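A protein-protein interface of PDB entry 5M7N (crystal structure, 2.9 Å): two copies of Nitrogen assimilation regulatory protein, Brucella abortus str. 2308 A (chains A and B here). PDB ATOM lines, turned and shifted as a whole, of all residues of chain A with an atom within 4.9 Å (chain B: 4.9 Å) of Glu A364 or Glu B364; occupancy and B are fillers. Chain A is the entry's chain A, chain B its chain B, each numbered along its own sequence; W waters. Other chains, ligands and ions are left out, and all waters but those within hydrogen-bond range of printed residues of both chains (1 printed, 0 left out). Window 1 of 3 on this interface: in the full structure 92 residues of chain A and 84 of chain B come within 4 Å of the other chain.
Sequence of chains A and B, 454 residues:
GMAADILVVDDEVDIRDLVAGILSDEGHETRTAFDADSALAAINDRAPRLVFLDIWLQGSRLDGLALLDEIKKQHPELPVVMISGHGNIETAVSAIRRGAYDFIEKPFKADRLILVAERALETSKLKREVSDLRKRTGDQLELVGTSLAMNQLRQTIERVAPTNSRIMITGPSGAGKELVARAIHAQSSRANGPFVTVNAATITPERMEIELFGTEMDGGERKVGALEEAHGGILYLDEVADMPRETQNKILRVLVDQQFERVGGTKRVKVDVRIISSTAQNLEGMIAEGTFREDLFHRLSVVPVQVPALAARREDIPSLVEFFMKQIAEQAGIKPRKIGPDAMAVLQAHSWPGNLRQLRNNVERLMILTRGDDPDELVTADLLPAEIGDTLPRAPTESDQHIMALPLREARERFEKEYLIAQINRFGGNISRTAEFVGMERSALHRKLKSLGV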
ATOM      1  N   ILE A 328     -21.150  12.239 -19.170  1.00  0.00           N
ATOM      2  CA  ILE A 328     -20.016  12.951 -18.540  1.00  0.00           C
ATOM      3  C   ILE A 328     -18.799  12.816 -19.465  1.00  0.00           C
ATOM      4  O   ILE A 328     -18.048  13.774 -19.627  1.00  0.00           O
ATOM      5  CB  ILE A 328     -19.639  12.480 -17.085  1.00  0.00           C
ATOM      6  CG1 ILE A 328     -20.870  12.183 -16.159  1.00  0.00           C
ATOM      7  CG2 ILE A 328     -18.670  13.459 -16.412  1.00  0.00           C
ATOM      8  CD1 ILE A 328     -21.899  13.271 -15.908  1.00  0.00           C
ATOM      9  N   GLN A 331     -18.930  15.209 -22.184  1.00  0.00           N
ATOM     10  CA  GLN A 331     -18.760  16.547 -21.629  1.00  0.00           C
ATOM     11  C   GLN A 331     -17.301  16.888 -21.249  1.00  0.00           C
ATOM     12  O   GLN A 331     -16.762  17.910 -21.707  1.00  0.00           O
ATOM     13  CB  GLN A 331     -19.625  16.711 -20.374  1.00  0.00           C
ATOM     14  CG  GLN A 331     -21.126  16.824 -20.591  1.00  0.00           C
ATOM     15  CD  GLN A 331     -21.857  16.938 -19.274  1.00  0.00           C
ATOM     16  OE1 GLN A 331     -21.324  16.657 -18.192  1.00  0.00           O
ATOM     17  NE2 GLN A 331     -23.097  17.369 -19.332  1.00  0.00           N
ATOM     18  N   ARG A 357     -31.780  14.252 -10.852  1.00  0.00           N
ATOM     19  CA  ARG A 357     -30.821  15.369 -10.788  1.00  0.00           C
ATOM     20  C   ARG A 357     -29.691  14.943  -9.838  1.00  0.00           C
ATOM     21  O   ARG A 357     -28.508  14.943 -10.228  1.00  0.00           O
ATOM     22  CB  ARG A 357     -31.494  16.658 -10.285  1.00  0.00           C
ATOM     23  CG  ARG A 357     -30.601  17.893 -10.336  1.00  0.00           C
ATOM     24  CD  ARG A 357     -31.430  19.169 -10.357  1.00  0.00           C
ATOM     25  NE  ARG A 357     -32.147  19.367 -11.623  1.00  0.00           N
ATOM     26  CZ  ARG A 357     -31.617  19.919 -12.713  1.00  0.00           C
ATOM     27  NH1 ARG A 357     -30.359  20.343 -12.711  1.00  0.00           N
ATOM     28  NH2 ARG A 357     -32.353  20.067 -13.812  1.00  0.00           N
ATOM     29  N   ARG A 360     -27.563  11.982 -11.139  1.00  0.00           N
ATOM     30  CA  ARG A 360     -26.640  12.535 -12.134  1.00  0.00           C
ATOM     31  C   ARG A 360     -25.455  13.226 -11.473  1.00  0.00           C
ATOM     32  O   ARG A 360     -24.306  12.930 -11.813  1.00  0.00           O
ATOM     33  CB  ARG A 360     -27.370  13.526 -13.031  1.00  0.00           C
ATOM     34  CG  ARG A 360     -26.708  13.732 -14.366  1.00  0.00           C
ATOM     35  CD  ARG A 360     -26.978  15.115 -14.891  1.00  0.00           C
ATOM     36  NE  ARG A 360     -25.949  16.019 -14.380  1.00  0.00           N
ATOM     37  CZ  ARG A 360     -24.777  16.219 -14.974  1.00  0.00           C
ATOM     38  NH1 ARG A 360     -24.493  15.629 -16.133  1.00  0.00           N
ATOM     39  NH2 ARG A 360     -23.885  17.035 -14.420  1.00  0.00           N
ATOM     40  N   ASN A 361     -25.735  14.138 -10.523  1.00  0.00           N
ATOM     41  CA  ASN A 361     -24.719  14.889  -9.785  1.00  0.00           C
ATOM     42  C   ASN A 361     -23.772  13.906  -9.090  1.00  0.00           C
ATOM     43  O   ASN A 361     -22.554  14.107  -9.104  1.00  0.00           O
ATOM     44  CB  ASN A 361     -25.407  15.823  -8.787  1.00  0.00           C
ATOM     45  CG  ASN A 361     -24.497  16.489  -7.805  1.00  0.00           C
ATOM     46  OD1 ASN A 361     -24.493  16.171  -6.608  1.00  0.00           O
ATOM     47  ND2 ASN A 361     -23.749  17.465  -8.279  1.00  0.00           N
ATOM     48  N   ASN A 362     -24.335  12.801  -8.566  1.00  0.00           N
ATOM     49  CA  ASN A 362     -23.572  11.762  -7.878  1.00  0.00           C
ATOM     50  C   ASN A 362     -22.701  10.953  -8.822  1.00  0.00           C
ATOM     51  O   ASN A 362     -21.573  10.601  -8.453  1.00  0.00           O
ATOM     52  CB  ASN A 362     -24.473  10.877  -7.021  1.00  0.00           C
ATOM     53  CG  ASN A 362     -24.509  11.389  -5.612  1.00  0.00           C
ATOM     54  OD1 ASN A 362     -23.578  11.155  -4.842  1.00  0.00           O
ATOM     55  ND2 ASN A 362     -25.504  12.212  -5.287  1.00  0.00           N
ATOM     56  N   VAL A 363     -23.209  10.682 -10.045  1.00  0.00           N
ATOM     57  CA  VAL A 363     -22.434   9.940 -11.054  1.00  0.00           C
ATOM     58  C   VAL A 363     -21.274  10.808 -11.511  1.00  0.00           C
ATOM     59  O   VAL A 363     -20.144  10.329 -11.506  1.00  0.00           O
ATOM     60  CB  VAL A 363     -23.270   9.339 -12.209  1.00  0.00           C
ATOM     61  CG1 VAL A 363     -22.388   8.544 -13.153  1.00  0.00           C
ATOM     62  CG2 VAL A 363     -24.379   8.445 -11.661  1.00  0.00           C
ATOM     63  N   GLU A 364     -21.544  12.110 -11.775  1.00  0.00           N
ATOM     64  CA  GLU A 364     -20.554  13.111 -12.154  1.00  0.00           C
ATOM     65  C   GLU A 364     -19.479  13.190 -11.057  1.00  0.00           C
ATOM     66  O   GLU A 364     -18.286  13.129 -11.375  1.00  0.00           O
ATOM     67  CB  GLU A 364     -21.236  14.466 -12.391  1.00  0.00           C
ATOM     68  CG  GLU A 364     -20.269  15.622 -12.583  1.00  0.00           C
ATOM     69  CD  GLU A 364     -20.876  16.948 -12.997  1.00  0.00           C
ATOM     70  OE1 GLU A 364     -21.686  17.519 -12.226  1.00  0.00           O
ATOM     71  OE2 GLU A 364     -20.515  17.429 -14.094  1.00  0.00           O
ATOM     72  N   ARG A 365     -19.893  13.257  -9.771  1.00  0.00           N
ATOM     73  CA  ARG A 365     -18.947  13.289  -8.648  1.00  0.00           C
ATOM     74  C   ARG A 365     -17.955  12.101  -8.690  1.00  0.00           C
ATOM     75  O   ARG A 365     -16.751  12.332  -8.666  1.00  0.00           O
ATOM     76  CB  ARG A 365     -19.680  13.362  -7.310  1.00  0.00           C
ATOM     77  CG  ARG A 365     -18.762  13.227  -6.142  1.00  0.00           C
ATOM     78  CD  ARG A 365     -19.195  14.019  -4.919  1.00  0.00           C
ATOM     79  NE  ARG A 365     -18.264  13.795  -3.808  1.00  0.00           N
ATOM     80  CZ  ARG A 365     -18.290  12.714  -3.041  1.00  0.00           C
ATOM     81  NH1 ARG A 365     -19.208  11.779  -3.238  1.00  0.00           N
ATOM     82  NH2 ARG A 365     -17.392  12.551  -2.085  1.00  0.00           N
ATOM     83  N   LEU A 366     -18.447  10.854  -8.811  1.00  0.00           N
ATOM     84  CA  LEU A 366     -17.587   9.662  -8.873  1.00  0.00           C
ATOM     85  C   LEU A 366     -16.587   9.749 -10.022  1.00  0.00           C
ATOM     86  O   LEU A 366     -15.418   9.434  -9.815  1.00  0.00           O
ATOM     87  CB  LEU A 366     -18.409   8.362  -8.978  1.00  0.00           C
ATOM     88  CG  LEU A 366     -19.394   8.037  -7.846  1.00  0.00           C
ATOM     89  CD1 LEU A 366     -20.429   7.070  -8.322  1.00  0.00           C
ATOM     90  CD2 LEU A 366     -18.682   7.512  -6.612  1.00  0.00           C
ATOM     91  N   MET A 367     -17.039  10.245 -11.210  1.00  0.00           N
ATOM     92  CA  MET A 367     -16.220  10.463 -12.420  1.00  0.00           C
ATOM     93  C   MET A 367     -15.056  11.423 -12.156  1.00  0.00           C
ATOM     94  O   MET A 367     -13.910  11.100 -12.484  1.00  0.00           O
ATOM     95  CB  MET A 367     -17.082  10.969 -13.595  1.00  0.00           C
ATOM     96  CG  MET A 367     -18.130   9.985 -14.075  1.00  0.00           C
ATOM     97  SD  MET A 367     -17.376   8.567 -14.892  1.00  0.00           S
ATOM     98  CE  MET A 367     -17.181   7.455 -13.522  1.00  0.00           C
ATOM     99  N   ILE A 368     -15.364  12.586 -11.532  1.00  0.00           N
ATOM    100  CA  ILE A 368     -14.394  13.596 -11.131  1.00  0.00           C
ATOM    101  C   ILE A 368     -13.436  12.956 -10.124  1.00  0.00           C
ATOM    102  O   ILE A 368     -12.242  12.888 -10.385  1.00  0.00           O
ATOM    103  CB  ILE A 368     -15.085  14.864 -10.548  1.00  0.00           C
ATOM    104  CG1 ILE A 368     -15.885  15.616 -11.627  1.00  0.00           C
ATOM    105  CG2 ILE A 368     -14.051  15.796  -9.891  1.00  0.00           C
ATOM    106  CD1 ILE A 368     -16.919  16.538 -11.082  1.00  0.00           C
ATOM    107  N   ILE B 328     -27.129  27.137 -12.201  1.00  0.00           N
ATOM    108  CA  ILE B 328     -27.977  26.012 -11.768  1.00  0.00           C
ATOM    109  C   ILE B 328     -29.422  26.469 -11.490  1.00  0.00           C
ATOM    110  O   ILE B 328     -30.330  25.651 -11.601  1.00  0.00           O
ATOM    111  CB  ILE B 328     -27.325  25.227 -10.577  1.00  0.00           C
ATOM    112  CG1 ILE B 328     -26.024  24.549 -11.023  1.00  0.00           C
ATOM    113  CG2 ILE B 328     -28.262  24.185  -9.954  1.00  0.00           C
ATOM    114  CD1 ILE B 328     -24.982  24.577 -10.048  1.00  0.00           C
ATOM    115  N   ARG B 360     -17.832  23.331  -9.427  1.00  0.00           N
ATOM    116  CA  ARG B 360     -19.200  23.420  -9.934  1.00  0.00           C
ATOM    117  C   ARG B 360     -20.090  22.286  -9.400  1.00  0.00           C
ATOM    118  O   ARG B 360     -21.167  22.569  -8.857  1.00  0.00           O
ATOM    119  CB  ARG B 360     -19.211  23.512 -11.468  1.00  0.00           C
ATOM    120  CG  ARG B 360     -20.611  23.711 -12.086  1.00  0.00           C
ATOM    121  CD  ARG B 360     -20.780  23.110 -13.480  1.00  0.00           C
ATOM    122  NE  ARG B 360     -20.498  21.670 -13.475  1.00  0.00           N
ATOM    123  CZ  ARG B 360     -19.433  21.113 -14.047  1.00  0.00           C
ATOM    124  NH1 ARG B 360     -18.552  21.861 -14.697  1.00  0.00           N
ATOM    125  NH2 ARG B 360     -19.238  19.806 -13.967  1.00  0.00           N
ATOM    126  N   ASN B 361     -19.610  21.014  -9.513  1.00  0.00           N
ATOM    127  CA  ASN B 361     -20.270  19.792  -9.026  1.00  0.00           C
ATOM    128  C   ASN B 361     -20.618  19.915  -7.541  1.00  0.00           C
ATOM    129  O   ASN B 361     -21.736  19.578  -7.138  1.00  0.00           O
ATOM    130  CB  ASN B 361     -19.380  18.564  -9.287  1.00  0.00           C
ATOM    131  CG  ASN B 361     -19.841  17.263  -8.653  1.00  0.00           C
ATOM    132  OD1 ASN B 361     -19.232  16.756  -7.693  1.00  0.00           O
ATOM    133  ND2 ASN B 361     -20.892  16.662  -9.201  1.00  0.00           N
ATOM    134  N   ASN B 362     -19.681  20.440  -6.743  1.00  0.00           N
ATOM    135  CA  ASN B 362     -19.869  20.654  -5.315  1.00  0.00           C
ATOM    136  C   ASN B 362     -20.926  21.705  -5.034  1.00  0.00           C
ATOM    137  O   ASN B 362     -21.754  21.488  -4.159  1.00  0.00           O
ATOM    138  CB  ASN B 362     -18.548  21.001  -4.649  1.00  0.00           C
ATOM    139  CG  ASN B 362     -17.797  19.765  -4.225  1.00  0.00           C
ATOM    140  OD1 ASN B 362     -18.202  19.073  -3.287  1.00  0.00           O
ATOM    141  ND2 ASN B 362     -16.710  19.437  -4.922  1.00  0.00           N
ATOM    142  N   VAL B 363     -20.928  22.815  -5.804  1.00  0.00           N
ATOM    143  CA  VAL B 363     -21.870  23.929  -5.670  1.00  0.00           C
ATOM    144  C   VAL B 363     -23.272  23.396  -5.964  1.00  0.00           C
ATOM    145  O   VAL B 363     -24.204  23.657  -5.202  1.00  0.00           O
ATOM    146  CB  VAL B 363     -21.462  25.144  -6.564  1.00  0.00           C
ATOM    147  CG1 VAL B 363     -22.538  26.235  -6.570  1.00  0.00           C
ATOM    148  CG2 VAL B 363     -20.112  25.730  -6.139  1.00  0.00           C
ATOM    149  N   GLU B 364     -23.392  22.600  -7.025  1.00  0.00           N
ATOM    150  CA  GLU B 364     -24.627  21.952  -7.435  1.00  0.00           C
ATOM    151  C   GLU B 364     -25.121  21.020  -6.342  1.00  0.00           C
ATOM    152  O   GLU B 364     -26.301  21.091  -5.995  1.00  0.00           O
ATOM    153  CB  GLU B 364     -24.403  21.145  -8.719  1.00  0.00           C
ATOM    154  CG  GLU B 364     -25.705  20.604  -9.282  1.00  0.00           C
ATOM    155  CD  GLU B 364     -25.624  19.737 -10.518  1.00  0.00           C
ATOM    156  OE1 GLU B 364     -24.501  19.487 -11.021  1.00  0.00           O
ATOM    157  OE2 GLU B 364     -26.708  19.325 -10.994  1.00  0.00           O
ATOM    158  N   ARG B 365     -24.227  20.140  -5.803  1.00  0.00           N
ATOM    159  CA  ARG B 365     -24.600  19.197  -4.746  1.00  0.00           C
ATOM    160  C   ARG B 365     -25.244  19.932  -3.576  1.00  0.00           C
ATOM    161  O   ARG B 365     -26.228  19.450  -3.016  1.00  0.00           O
ATOM    162  CB  ARG B 365     -23.395  18.377  -4.269  1.00  0.00           C
ATOM    163  CG  ARG B 365     -23.777  17.284  -3.274  1.00  0.00           C
ATOM    164  CD  ARG B 365     -22.581  16.506  -2.764  1.00  0.00           C
ATOM    165  NE  ARG B 365     -22.790  16.080  -1.384  1.00  0.00           N
ATOM    166  CZ  ARG B 365     -22.472  16.816  -0.329  1.00  0.00           C
ATOM    167  NH1 ARG B 365     -21.902  18.006  -0.485  1.00  0.00           N
ATOM    168  NH2 ARG B 365     -22.725  16.373   0.895  1.00  0.00           N
ATOM    169  N   LEU B 366     -24.711  21.120  -3.250  1.00  0.00           N
ATOM    170  CA  LEU B 366     -25.221  21.961  -2.180  1.00  0.00           C
ATOM    171  C   LEU B 366     -26.606  22.492  -2.507  1.00  0.00           C
ATOM    172  O   LEU B 366     -27.460  22.477  -1.622  1.00  0.00           O
ATOM    173  CB  LEU B 366     -24.229  23.074  -1.809  1.00  0.00           C
ATOM    174  CG  LEU B 366     -22.870  22.594  -1.252  1.00  0.00           C
ATOM    175  CD1 LEU B 366     -21.932  23.746  -1.022  1.00  0.00           C
ATOM    176  CD2 LEU B 366     -23.024  21.757   0.022  1.00  0.00           C
ATOM    177  N   MET B 367     -26.858  22.875  -3.786  1.00  0.00           N
ATOM    178  CA  MET B 367     -28.159  23.376  -4.256  1.00  0.00           C
ATOM    179  C   MET B 367     -29.241  22.319  -4.097  1.00  0.00           C
ATOM    180  O   MET B 367     -30.339  22.625  -3.641  1.00  0.00           O
ATOM    181  CB  MET B 367     -28.085  23.799  -5.728  1.00  0.00           C
ATOM    182  CG  MET B 367     -27.175  24.967  -5.991  1.00  0.00           C
ATOM    183  SD  MET B 367     -27.741  26.481  -5.190  1.00  0.00           S
ATOM    184  CE  MET B 367     -29.101  26.937  -6.258  1.00  0.00           C
ATOM    185  N   ILE B 368     -28.919  21.074  -4.472  1.00  0.00           N
ATOM    186  CA  ILE B 368     -29.805  19.916  -4.406  1.00  0.00           C
ATOM    187  C   ILE B 368     -30.160  19.596  -2.946  1.00  0.00           C
ATOM    188  O   ILE B 368     -31.342  19.529  -2.615  1.00  0.00           O
ATOM    189  CB  ILE B 368     -29.177  18.692  -5.143  1.00  0.00           C
ATOM    190  CG1 ILE B 368     -28.970  18.976  -6.644  1.00  0.00           C
ATOM    191  CG2 ILE B 368     -30.006  17.429  -4.932  1.00  0.00           C
ATOM    192  CD1 ILE B 368     -27.870  18.157  -7.294  1.00  0.00           C
HETATM  193  O   HOH W   1     -27.319  16.951 -12.048  1.00  0.00           O
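Printed residues of chain B within 4 Å of Asn A361: Asn B361 (3.0 Å), Glu B364 (3.5 Å), Arg B365 (3.4 Å) and Ile B368 (3.7 Å). Glu A364 touches just these residues of chain B: Arg B360, Asn B361 and Glu B364. Printed residues of chain A within 4 Å of Arg B360: Glu A364 (2.7 Å). Glu B364 touches just these residues of chain A: Asn A361 and Glu A364. Met B367 touches none of the printed residues of chain A. Of the printed residues of chain A, Ile B368 touches Asn A361. The nearest printed residue of chain B that does not touch Glu A364 is Asn B362 (6.5 Å). The nearest residue of chain A that does not touch Glu B364 is Arg A357 (4.2 Å). The nearest printed residue of chain B that does not touch Arg A365 is Arg B365 (4.7 Å).
Asn A361 touches Arg B365 (OD1 to CB, 3.4 Å). CD1 of Ile B368 touches CB of Asn A361, at 3.7 Å. OE1 of Glu A364 touches OE1 of Glu B364 (3.6 Å). Asn B361 touches Arg A365 (OD1 to CB, 3.4 Å). CD1 of Ile A368 touches CB of Asn B361, 3.7 Å away.
The guanidinium group (NH2) of Arg A360 is in salt-bridge range of the side-chain carboxylate (OE1) of Glu A364 (3.1 Å).
Of the 10 printed residues of chain B, 5 touch a printed residue of chain A. Hydrophobic or aromatic side chains of chain B within 4 Å of the printed part of chain A: Ile B368. Among the printed residues, 9 pairs touch across the chains. Among the printed residues, Asp or Glu carboxylates within 4 Å of a Lys or Arg side-chain nitrogen of the other chain: Glu A364 with Arg B360 (2.7 Å).
Asn A361 touches Arg B365, and with the chains exchanged Arg A365 touches Asn B361. Asn A361 touches Ile B368, and with the chains exchanged Ile A368 touches Asn B361. Glu A364 touches Arg B360, but with the chains exchanged Arg A360 does not touch Glu B364 (4.2 Å). Glu A364 touches its own counterpart, Glu B364. Positions printed for both chains: 328, 360, 361, 362, 363, 364, 365, 366, 367 and 368. Of the 9 pairs that touch across the chains among the printed residues, 8 have their exchanged pair printed and touching as well.
O of Asn A361 is in hydrogen-bond range of ND2 of Asn B361, 3.0 Å away. The side-chain amide nitrogen of Asn A361 sits at hydrogen-bond distance from the side-chain carboxylate of Glu B364 (3.5 Å). OE2 of Glu A364 lies within salt-bridge range of NH2 of Arg B360. The side-chain carboxylate (OE1) of Glu A364 lies within hydrogen-bond range of the side-chain amide nitrogen (ND2) of Asn B361 (3.2 Å).
Water W1 lies within hydrogen-bond range of OE2 of Glu B364, NE of Arg A360 and O of Arg A357.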
